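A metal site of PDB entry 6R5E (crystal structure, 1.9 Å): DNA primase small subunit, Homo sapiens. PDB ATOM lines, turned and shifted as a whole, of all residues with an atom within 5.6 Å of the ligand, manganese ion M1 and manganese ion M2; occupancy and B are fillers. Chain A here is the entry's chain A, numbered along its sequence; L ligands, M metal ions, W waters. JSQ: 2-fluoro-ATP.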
ATOM      1  N   TYR A  57      -9.519  -0.863 -12.480  1.00  0.00           N
ATOM      2  CA  TYR A  57      -8.795  -1.211 -11.272  1.00  0.00           C
ATOM      3  C   TYR A  57      -8.634   0.001 -10.358  1.00  0.00           C
ATOM      4  O   TYR A  57      -8.777   1.145 -10.781  1.00  0.00           O
ATOM      5  CB  TYR A  57      -7.416  -1.823 -11.578  1.00  0.00           C
ATOM      6  CG  TYR A  57      -6.439  -0.909 -12.295  1.00  0.00           C
ATOM      7  CD1 TYR A  57      -6.520  -0.720 -13.669  1.00  0.00           C
ATOM      8  CD2 TYR A  57      -5.435  -0.253 -11.600  1.00  0.00           C
ATOM      9  CE1 TYR A  57      -5.620   0.110 -14.329  1.00  0.00           C
ATOM     10  CE2 TYR A  57      -4.534   0.580 -12.251  1.00  0.00           C
ATOM     11  CZ  TYR A  57      -4.638   0.750 -13.615  1.00  0.00           C
ATOM     12  OH  TYR A  57      -3.746   1.580 -14.264  1.00  0.00           O
ATOM     13  N   ARG A  59      -6.147   1.609  -7.236  1.00  0.00           N
ATOM     14  CA  ARG A  59      -4.869   1.590  -6.532  1.00  0.00           C
ATOM     15  C   ARG A  59      -5.058   1.953  -5.059  1.00  0.00           C
ATOM     16  O   ARG A  59      -6.077   2.504  -4.654  1.00  0.00           O
ATOM     17  CB  ARG A  59      -3.871   2.589  -7.154  1.00  0.00           C
ATOM     18  CG  ARG A  59      -3.381   2.297  -8.570  1.00  0.00           C
ATOM     19  CD  ARG A  59      -2.420   1.117  -8.659  1.00  0.00           C
ATOM     20  NE  ARG A  59      -1.300   1.183  -7.728  1.00  0.00           N
ATOM     21  CZ  ARG A  59      -0.083   1.634  -8.020  1.00  0.00           C
ATOM     22  NH1 ARG A  59       0.212   2.070  -9.246  1.00  0.00           N
ATOM     23  NH2 ARG A  59       0.859   1.655  -7.090  1.00  0.00           N
ATOM     24  N   LYS A  80      -9.077  -9.731 -10.070  1.00  0.00           N
ATOM     25  CA  LYS A  80      -7.653  -9.919  -9.839  1.00  0.00           C
ATOM     26  C   LYS A  80      -7.243  -9.096  -8.634  1.00  0.00           C
ATOM     27  O   LYS A  80      -7.814  -8.038  -8.362  1.00  0.00           O
ATOM     28  CB  LYS A  80      -6.868  -9.506 -11.096  1.00  0.00           C
ATOM     29  CG  LYS A  80      -5.393  -9.851 -11.101  1.00  0.00           C
ATOM     30  CD  LYS A  80      -4.799  -9.511 -12.466  1.00  0.00           C
ATOM     31  CE  LYS A  80      -4.598  -8.012 -12.650  1.00  0.00           C
ATOM     32  NZ  LYS A  80      -3.279  -7.585 -12.100  1.00  0.00           N
ATOM     33  N   ASP A  82      -3.682  -7.590  -6.820  1.00  0.00           N
ATOM     34  CA  ASP A  82      -2.249  -7.338  -6.855  1.00  0.00           C
ATOM     35  C   ASP A  82      -1.774  -6.814  -5.505  1.00  0.00           C
ATOM     36  O   ASP A  82      -2.474  -6.060  -4.836  1.00  0.00           O
ATOM     37  CB  ASP A  82      -1.891  -6.313  -7.936  1.00  0.00           C
ATOM     38  CG  ASP A  82      -2.218  -6.798  -9.334  1.00  0.00           C
ATOM     39  OD1 ASP A  82      -1.827  -7.933  -9.670  1.00  0.00           O
ATOM     40  OD2 ASP A  82      -2.853  -6.050 -10.098  1.00  0.00           O
ATOM     41  N   ASP A 112       9.440 -12.179 -11.857  1.00  0.00           N
ATOM     42  CA  ASP A 112       8.351 -12.553 -12.765  1.00  0.00           C
ATOM     43  C   ASP A 112       9.003 -13.080 -14.034  1.00  0.00           C
ATOM     44  O   ASP A 112       9.719 -12.347 -14.709  1.00  0.00           O
ATOM     45  CB  ASP A 112       7.432 -11.355 -13.060  1.00  0.00           C
ATOM     46  CG  ASP A 112       6.450 -11.607 -14.223  1.00  0.00           C
ATOM     47  OD1 ASP A 112       5.862 -12.699 -14.335  1.00  0.00           O
ATOM     48  OD2 ASP A 112       6.249 -10.666 -15.016  1.00  0.00           O
ATOM     49  N   ILE A 113       8.740 -14.348 -14.355  1.00  0.00           N
ATOM     50  CA  ILE A 113       9.309 -15.002 -15.519  1.00  0.00           C
ATOM     51  C   ILE A 113       8.171 -15.353 -16.462  1.00  0.00           C
ATOM     52  O   ILE A 113       7.176 -15.952 -16.049  1.00  0.00           O
ATOM     53  CB  ILE A 113      10.114 -16.261 -15.150  1.00  0.00           C
ATOM     54  CG1 ILE A 113      11.070 -15.941 -13.988  1.00  0.00           C
ATOM     55  CG2 ILE A 113      10.862 -16.787 -16.374  1.00  0.00           C
ATOM     56  CD1 ILE A 113      12.131 -16.986 -13.728  1.00  0.00           C
ATOM     57  N   ASP A 114       8.324 -14.971 -17.732  1.00  0.00           N
ATOM     58  CA  ASP A 114       7.289 -15.142 -18.750  1.00  0.00           C
ATOM     59  C   ASP A 114       7.840 -16.015 -19.865  1.00  0.00           C
ATOM     60  O   ASP A 114       8.879 -15.692 -20.449  1.00  0.00           O
ATOM     61  CB  ASP A 114       6.834 -13.787 -19.298  1.00  0.00           C
ATOM     62  CG  ASP A 114       6.149 -12.914 -18.247  1.00  0.00           C
ATOM     63  OD1 ASP A 114       5.496 -13.472 -17.332  1.00  0.00           O
ATOM     64  OD2 ASP A 114       6.247 -11.668 -18.332  1.00  0.00           O
ATOM     65  N   SER A 163       2.043 -18.382 -12.114  1.00  0.00           N
ATOM     66  CA  SER A 163       1.355 -17.124 -12.396  1.00  0.00           C
ATOM     67  C   SER A 163      -0.038 -17.308 -12.975  1.00  0.00           C
ATOM     68  O   SER A 163      -0.800 -16.342 -13.039  1.00  0.00           O
ATOM     69  CB  SER A 163       2.201 -16.249 -13.335  1.00  0.00           C
ATOM     70  OG  SER A 163       2.440 -16.879 -14.577  1.00  0.00           O
ATOM     71  N   GLY A 164      -0.386 -18.521 -13.394  1.00  0.00           N
ATOM     72  CA  GLY A 164      -1.724 -18.796 -13.869  1.00  0.00           C
ATOM     73  C   GLY A 164      -1.875 -18.874 -15.375  1.00  0.00           C
ATOM     74  O   GLY A 164      -2.925 -19.307 -15.848  1.00  0.00           O
ATOM     75  N   ARG A 165      -0.858 -18.447 -16.133  1.00  0.00           N
ATOM     76  CA  ARG A 165      -0.950 -18.539 -17.586  1.00  0.00           C
ATOM     77  C   ARG A 165       0.373 -18.932 -18.232  1.00  0.00           C
ATOM     78  O   ARG A 165       0.442 -19.973 -18.896  1.00  0.00           O
ATOM     79  CB  ARG A 165      -1.457 -17.207 -18.165  1.00  0.00           C
ATOM     80  CG  ARG A 165      -1.695 -17.253 -19.664  1.00  0.00           C
ATOM     81  CD  ARG A 165      -2.334 -15.970 -20.183  1.00  0.00           C
ATOM     82  NE  ARG A 165      -1.483 -14.801 -19.981  1.00  0.00           N
ATOM     83  CZ  ARG A 165      -1.424 -13.751 -20.791  1.00  0.00           C
ATOM     84  NH1 ARG A 165      -2.166 -13.709 -21.898  1.00  0.00           N
ATOM     85  NH2 ARG A 165      -0.620 -12.739 -20.517  1.00  0.00           N
ATOM     86  N   ARG A 166       1.446 -18.140 -18.050  1.00  0.00           N
ATOM     87  CA  ARG A 166       2.616 -18.325 -18.899  1.00  0.00           C
ATOM     88  C   ARG A 166       3.950 -18.327 -18.152  1.00  0.00           C
ATOM     89  O   ARG A 166       4.999 -18.175 -18.782  1.00  0.00           O
ATOM     90  CB  ARG A 166       2.650 -17.250 -19.983  1.00  0.00           C
ATOM     91  CG  ARG A 166       2.572 -15.856 -19.414  1.00  0.00           C
ATOM     92  CD  ARG A 166       2.770 -14.787 -20.456  1.00  0.00           C
ATOM     93  NE  ARG A 166       2.872 -13.484 -19.814  1.00  0.00           N
ATOM     94  CZ  ARG A 166       3.118 -12.341 -20.450  1.00  0.00           C
ATOM     95  NH1 ARG A 166       3.289 -12.331 -21.768  1.00  0.00           N
ATOM     96  NH2 ARG A 166       3.185 -11.208 -19.756  1.00  0.00           N
ATOM     97  N   GLY A 167       3.956 -18.522 -16.834  1.00  0.00           N
ATOM     98  CA  GLY A 167       5.235 -18.614 -16.147  1.00  0.00           C
ATOM     99  C   GLY A 167       5.099 -18.694 -14.636  1.00  0.00           C
ATOM    100  O   GLY A 167       4.111 -19.219 -14.111  1.00  0.00           O
ATOM    101  N   VAL A 168       6.118 -18.170 -13.947  1.00  0.00           N
ATOM    102  CA  VAL A 168       6.226 -18.302 -12.501  1.00  0.00           C
ATOM    103  C   VAL A 168       6.661 -16.989 -11.858  1.00  0.00           C
ATOM    104  O   VAL A 168       7.256 -16.116 -12.499  1.00  0.00           O
ATOM    105  CB  VAL A 168       7.216 -19.417 -12.082  1.00  0.00           C
ATOM    106  CG1 VAL A 168       6.786 -20.763 -12.659  1.00  0.00           C
ATOM    107  CG2 VAL A 168       8.647 -19.067 -12.515  1.00  0.00           C
ATOM    108  N   HIS A 169       6.369 -16.888 -10.560  1.00  0.00           N
ATOM    109  CA  HIS A 169       6.787 -15.772  -9.728  1.00  0.00           C
ATOM    110  C   HIS A 169       7.622 -16.307  -8.578  1.00  0.00           C
ATOM    111  O   HIS A 169       7.480 -17.457  -8.173  1.00  0.00           O
ATOM    112  CB  HIS A 169       5.587 -15.019  -9.157  1.00  0.00           C
ATOM    113  CG  HIS A 169       4.708 -14.382 -10.180  1.00  0.00           C
ATOM    114  ND1 HIS A 169       3.403 -14.046  -9.909  1.00  0.00           N
ATOM    115  CD2 HIS A 169       4.940 -14.014 -11.462  1.00  0.00           C
ATOM    116  CE1 HIS A 169       2.861 -13.494 -10.981  1.00  0.00           C
ATOM    117  NE2 HIS A 169       3.775 -13.462 -11.941  1.00  0.00           N
ATOM    118  N   ASP A 309      11.701 -10.955 -16.256  1.00  0.00           N
ATOM    119  CA  ASP A 309      11.031  -9.690 -16.541  1.00  0.00           C
ATOM    120  C   ASP A 309      11.604  -8.691 -15.541  1.00  0.00           C
ATOM    121  O   ASP A 309      11.097  -8.528 -14.429  1.00  0.00           O
ATOM    122  CB  ASP A 309       9.519  -9.826 -16.424  1.00  0.00           C
ATOM    123  CG  ASP A 309       8.770  -8.632 -16.998  1.00  0.00           C
ATOM    124  OD1 ASP A 309       9.395  -7.572 -17.175  1.00  0.00           O
ATOM    125  OD2 ASP A 309       7.546  -8.764 -17.257  1.00  0.00           O
ATOM    126  N   VAL A 312      10.022  -5.847 -13.146  1.00  0.00           N
ATOM    127  CA  VAL A 312       9.202  -6.273 -12.020  1.00  0.00           C
ATOM    128  C   VAL A 312      10.031  -6.335 -10.742  1.00  0.00           C
ATOM    129  O   VAL A 312       9.513  -6.092  -9.647  1.00  0.00           O
ATOM    130  CB  VAL A 312       8.553  -7.641 -12.337  1.00  0.00           C
ATOM    131  CG1 VAL A 312       7.650  -8.098 -11.194  1.00  0.00           C
ATOM    132  CG2 VAL A 312       7.768  -7.568 -13.644  1.00  0.00           C
ATOM    133  N   HIS A 318       6.489  -1.638  -7.398  1.00  0.00           N
ATOM    134  CA  HIS A 318       5.851  -2.431  -8.447  1.00  0.00           C
ATOM    135  C   HIS A 318       4.854  -3.435  -7.876  1.00  0.00           C
ATOM    136  O   HIS A 318       5.136  -4.133  -6.900  1.00  0.00           O
ATOM    137  CB  HIS A 318       6.911  -3.154  -9.263  1.00  0.00           C
ATOM    138  CG  HIS A 318       6.454  -3.560 -10.625  1.00  0.00           C
ATOM    139  ND1 HIS A 318       5.586  -4.607 -10.849  1.00  0.00           N
ATOM    140  CD2 HIS A 318       6.742  -3.045 -11.847  1.00  0.00           C
ATOM    141  CE1 HIS A 318       5.364  -4.730 -12.152  1.00  0.00           C
ATOM    142  NE2 HIS A 318       6.056  -3.788 -12.782  1.00  0.00           N
ATOM    143  N   LEU A 319       3.693  -3.514  -8.512  1.00  0.00           N
ATOM    144  CA  LEU A 319       2.667  -4.475  -8.156  1.00  0.00           C
ATOM    145  C   LEU A 319       2.962  -5.832  -8.767  1.00  0.00           C
ATOM    146  O   LEU A 319       3.579  -5.943  -9.832  1.00  0.00           O
ATOM    147  CB  LEU A 319       1.289  -3.991  -8.626  1.00  0.00           C
ATOM    148  CG  LEU A 319       0.764  -2.665  -8.082  1.00  0.00           C
ATOM    149  CD1 LEU A 319      -0.423  -2.165  -8.902  1.00  0.00           C
ATOM    150  CD2 LEU A 319       0.358  -2.811  -6.621  1.00  0.00           C
ATOM    151  N   LEU A 320       2.519  -6.887  -8.084  1.00  0.00           N
ATOM    152  CA  LEU A 320       2.602  -8.243  -8.614  1.00  0.00           C
ATOM    153  C   LEU A 320       1.354  -9.007  -8.194  1.00  0.00           C
ATOM    154  O   LEU A 320       0.863  -8.859  -7.078  1.00  0.00           O
ATOM    155  CB  LEU A 320       3.859  -8.980  -8.128  1.00  0.00           C
ATOM    156  CG  LEU A 320       4.110 -10.367  -8.735  1.00  0.00           C
ATOM    157  CD1 LEU A 320       4.278 -10.285 -10.250  1.00  0.00           C
ATOM    158  CD2 LEU A 320       5.350 -11.013  -8.122  1.00  0.00           C
ATOM    159  N   LYS A 321       0.845  -9.820  -9.129  1.00  0.00           N
ATOM    160  CA  LYS A 321      -0.350 -10.612  -8.864  1.00  0.00           C
ATOM    161  C   LYS A 321      -0.197 -11.445  -7.605  1.00  0.00           C
ATOM    162  O   LYS A 321       0.812 -12.127  -7.419  1.00  0.00           O
ATOM    163  CB  LYS A 321      -0.637 -11.526 -10.057  1.00  0.00           C
ATOM    164  CG  LYS A 321      -2.085 -11.545 -10.509  1.00  0.00           C
ATOM    165  CD  LYS A 321      -2.765 -12.870 -10.232  1.00  0.00           C
ATOM    166  CE  LYS A 321      -2.765 -13.763 -11.467  1.00  0.00           C
ATOM    167  NZ  LYS A 321      -1.396 -14.091 -11.938  1.00  0.00           N
ATOM    168  N   HIS A 327      -6.184 -15.916 -12.312  1.00  0.00           N
ATOM    169  CA  HIS A 327      -5.756 -15.286 -13.544  1.00  0.00           C
ATOM    170  C   HIS A 327      -6.980 -15.168 -14.437  1.00  0.00           C
ATOM    171  O   HIS A 327      -7.482 -16.206 -14.918  1.00  0.00           O
ATOM    172  CB  HIS A 327      -4.666 -16.103 -14.232  1.00  0.00           C
ATOM    173  CG  HIS A 327      -3.925 -15.337 -15.293  1.00  0.00           C
ATOM    174  ND1 HIS A 327      -4.573 -14.723 -16.348  1.00  0.00           N
ATOM    175  CD2 HIS A 327      -2.607 -15.082 -15.449  1.00  0.00           C
ATOM    176  CE1 HIS A 327      -3.675 -14.120 -17.107  1.00  0.00           C
ATOM    177  NE2 HIS A 327      -2.481 -14.316 -16.589  1.00  0.00           N
HETATM  178  N3  JSQ L   1       0.792  -3.220 -12.724  1.00  0.00           N
HETATM  179  C2  JSQ L   1       0.288  -2.067 -13.089  1.00  0.00           C
HETATM  180  C5  JSQ L   1       0.094  -3.888 -14.954  1.00  0.00           C
HETATM  181  C4  JSQ L   1       0.660  -4.113 -13.713  1.00  0.00           C
HETATM  182  C6  JSQ L   1      -0.401  -2.601 -15.198  1.00  0.00           C
HETATM  183  F2  JSQ L   1       0.369  -1.103 -12.165  1.00  0.00           F
HETATM  184  C1' JSQ L   1       1.693  -6.169 -12.638  1.00  0.00           C
HETATM  185  C2' JSQ L   1       0.736  -7.226 -12.072  1.00  0.00           C
HETATM  186  C3' JSQ L   1       1.242  -8.508 -12.737  1.00  0.00           C
HETATM  187  C4' JSQ L   1       2.729  -8.251 -12.865  1.00  0.00           C
HETATM  188  C5' JSQ L   1       3.406  -9.038 -13.957  1.00  0.00           C
HETATM  189  C8  JSQ L   1       0.705  -5.918 -14.942  1.00  0.00           C
HETATM  190  N1  JSQ L   1      -0.281  -1.681 -14.217  1.00  0.00           N
HETATM  191  N6  JSQ L   1      -0.974  -2.209 -16.338  1.00  0.00           N
HETATM  192  N7  JSQ L   1       0.129  -5.046 -15.722  1.00  0.00           N
HETATM  193  N9  JSQ L   1       1.074  -5.416 -13.724  1.00  0.00           N
HETATM  194  O1A JSQ L   1       1.770  -9.610 -17.458  1.00  0.00           O
HETATM  195  O1B JSQ L   1       0.630 -12.059 -13.293  1.00  0.00           O
HETATM  196  O1G JSQ L   1       0.060 -13.869 -17.765  1.00  0.00           O
HETATM  197  O2' JSQ L   1       0.785  -7.243 -10.652  1.00  0.00           O
HETATM  198  O2A JSQ L   1       3.603 -10.874 -16.359  1.00  0.00           O
HETATM  199  O2B JSQ L   1       2.824 -12.665 -14.402  1.00  0.00           O
HETATM  200  O2G JSQ L   1       2.406 -13.665 -17.014  1.00  0.00           O
HETATM  201  O3' JSQ L   1       0.988  -9.636 -11.905  1.00  0.00           O
HETATM  202  O3A JSQ L   1       1.245 -10.916 -15.408  1.00  0.00           O
HETATM  203  O3B JSQ L   1       0.560 -13.374 -15.382  1.00  0.00           O
HETATM  204  O3G JSQ L   1       1.080 -15.614 -16.310  1.00  0.00           O
HETATM  205  O4' JSQ L   1       2.831  -6.842 -13.158  1.00  0.00           O
HETATM  206  O5' JSQ L   1       2.691  -8.821 -15.194  1.00  0.00           O
HETATM  207  PA  JSQ L   1       2.335 -10.032 -16.156  1.00  0.00           P
HETATM  208  PB  JSQ L   1       1.337 -12.262 -14.556  1.00  0.00           P
HETATM  209  PG  JSQ L   1       1.021 -14.147 -16.697  1.00  0.00           P
HETATM  210 MN    MN M   1       5.728  -9.973 -17.015  1.00  0.00          MN
HETATM  211 MN    MN M   2       4.218 -12.969 -15.780  1.00  0.00          MN
HETATM  212  O   HOH W   1       5.163  -7.688 -16.271  1.00  0.00           O
HETATM  213  O   HOH W   2       4.632  -8.585 -18.729  1.00  0.00           O
HETATM  214  O   HOH W   3       3.113  -1.828 -11.057  1.00  0.00           O
HETATM  215  O   HOH W   4       4.493 -14.994 -15.092  1.00  0.00           O
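Merely in contact with manganese ion M1: Arg 166.
Of the 21 residues printed, 4 come within 4 Å of manganese ion M1.
Water W2 bridges NH2 of Arg 166 and O1A of the ligand.
Water W4 bridges the side-chain hydroxyl (OG) of Ser 163 (2.8 Å) and the backbone carbonyl oxygen (O) of Ile 113 (3.0 Å).
Water W3 bridges the backbone NH (N) of Leu 319 (3.1 Å) and a nitrogen (N3) of the ligand (3.2 Å).
The guanidinium group of Arg 166 lies close to the side-chain carboxylate of Asp 114 (3.4 Å).
A ring nitrogen (NE2) of His 169 sits close to the side-chain carboxylate of Asp 112, at 3.3 Å.
The backbone carbonyl oxygen of Ser 163 is in hydrogen-bond range of the side-chain amino group of Lys 321 (2.6 Å).
O of Gly 167 sits at hydrogen-bond distance from OG of Ser 163 (2.9 Å).
The backbone NH (N) of Lys 321 sits close to the side-chain carboxylate (OD1) of Asp 82, 3.3 Å away.
The side-chain amino group (NZ) of Lys 80 lies within salt-bridge range of the side-chain carboxylate (OD2) of Asp 82, at 2.6 Å.
Manganese ion M1 is bound by the side-chain carboxylate (OD2) of Asp 112 (2.2 Å), the side-chain carboxylate (OD2) of Asp 309 (2.2 Å), the side-chain carboxylate (OD2) of Asp 114 (2.2 Å), an oxygen (O2A) of the ligand (2.4 Å), water W2 (2.5 Å) and water W1 (2.5 Å).
The side-chain hydroxyl (OG) of Ser 163 is in hydrogen-bond range of an oxygen (O3G) of the ligand, 2.5 Å away.
A ring nitrogen (NE2) of His 169 sits close to an oxygen (O2B) of the ligand.
An oxygen (O3') of the ligand is in hydrogen-bond range of the backbone NH of Lys 321 (2.8 Å).
The side-chain amino group (NZ) of Lys 321 lies within salt-bridge range of an oxygen (O1B) of the ligand (3.2 Å).
An oxygen (O1G) of the ligand is in hydrogen-bond range of a ring nitrogen (NE2) of His 327, at 2.8 Å.
N of Arg 166 lies within hydrogen-bond range of O3G of the ligand, 3.1 Å away.
O1A of the ligand is in salt-bridge range of NH2 of Arg 166, 3.1 Å away.
An oxygen (O3G) of the ligand sits at hydrogen-bond distance from the backbone NH (N) of Arg 165, 3.4 Å away.
NE of Arg 165 is in salt-bridge range of O1G of the ligand (2.9 Å).
O2' of the ligand is in hydrogen-bond range of OD1 of Asp 82 (2.9 Å).
N of Leu 320 lies close to O2' of the ligand (3.1 Å).
The backbone carbonyl oxygen (O) of Leu 319 is in hydrogen-bond range of an oxygen (O2') of the ligand, at 3.2 Å.
NE2 of His 169 touches manganese ion M2, 3.9 Å away.
Of the 21 residues printed, 3 come within 4 Å of manganese ion M2.
The nearest printed residue that does not touch manganese ion M2 is Ile 113 (4.2 Å).
Manganese ion M2 is bound by O2B of the ligand (2.0 Å), OD1 of Asp 114 (2.1 Å), water W4 (2.2 Å), OD1 of Asp 112 (2.2 Å), O2A of the ligand (2.3 Å) and O2G of the ligand (2.3 Å).
Manganese ion M2 has six donor atoms within binding distance.
His 318 touches the ligand (CE1 to O4', 3.4 Å).
Hydrophobic or aromatic side chains within 4 Å of the ligand: His 169, His 318, Leu 319, Leu 320 and His 327.
12 residues have an atom within 4 Å of the ligand: Asp 82, Asp 112, Asp 114, Ser 163, Arg 165, Arg 166, His 169, His 318, Leu 319, Leu 320, Lys 321 and His 327.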
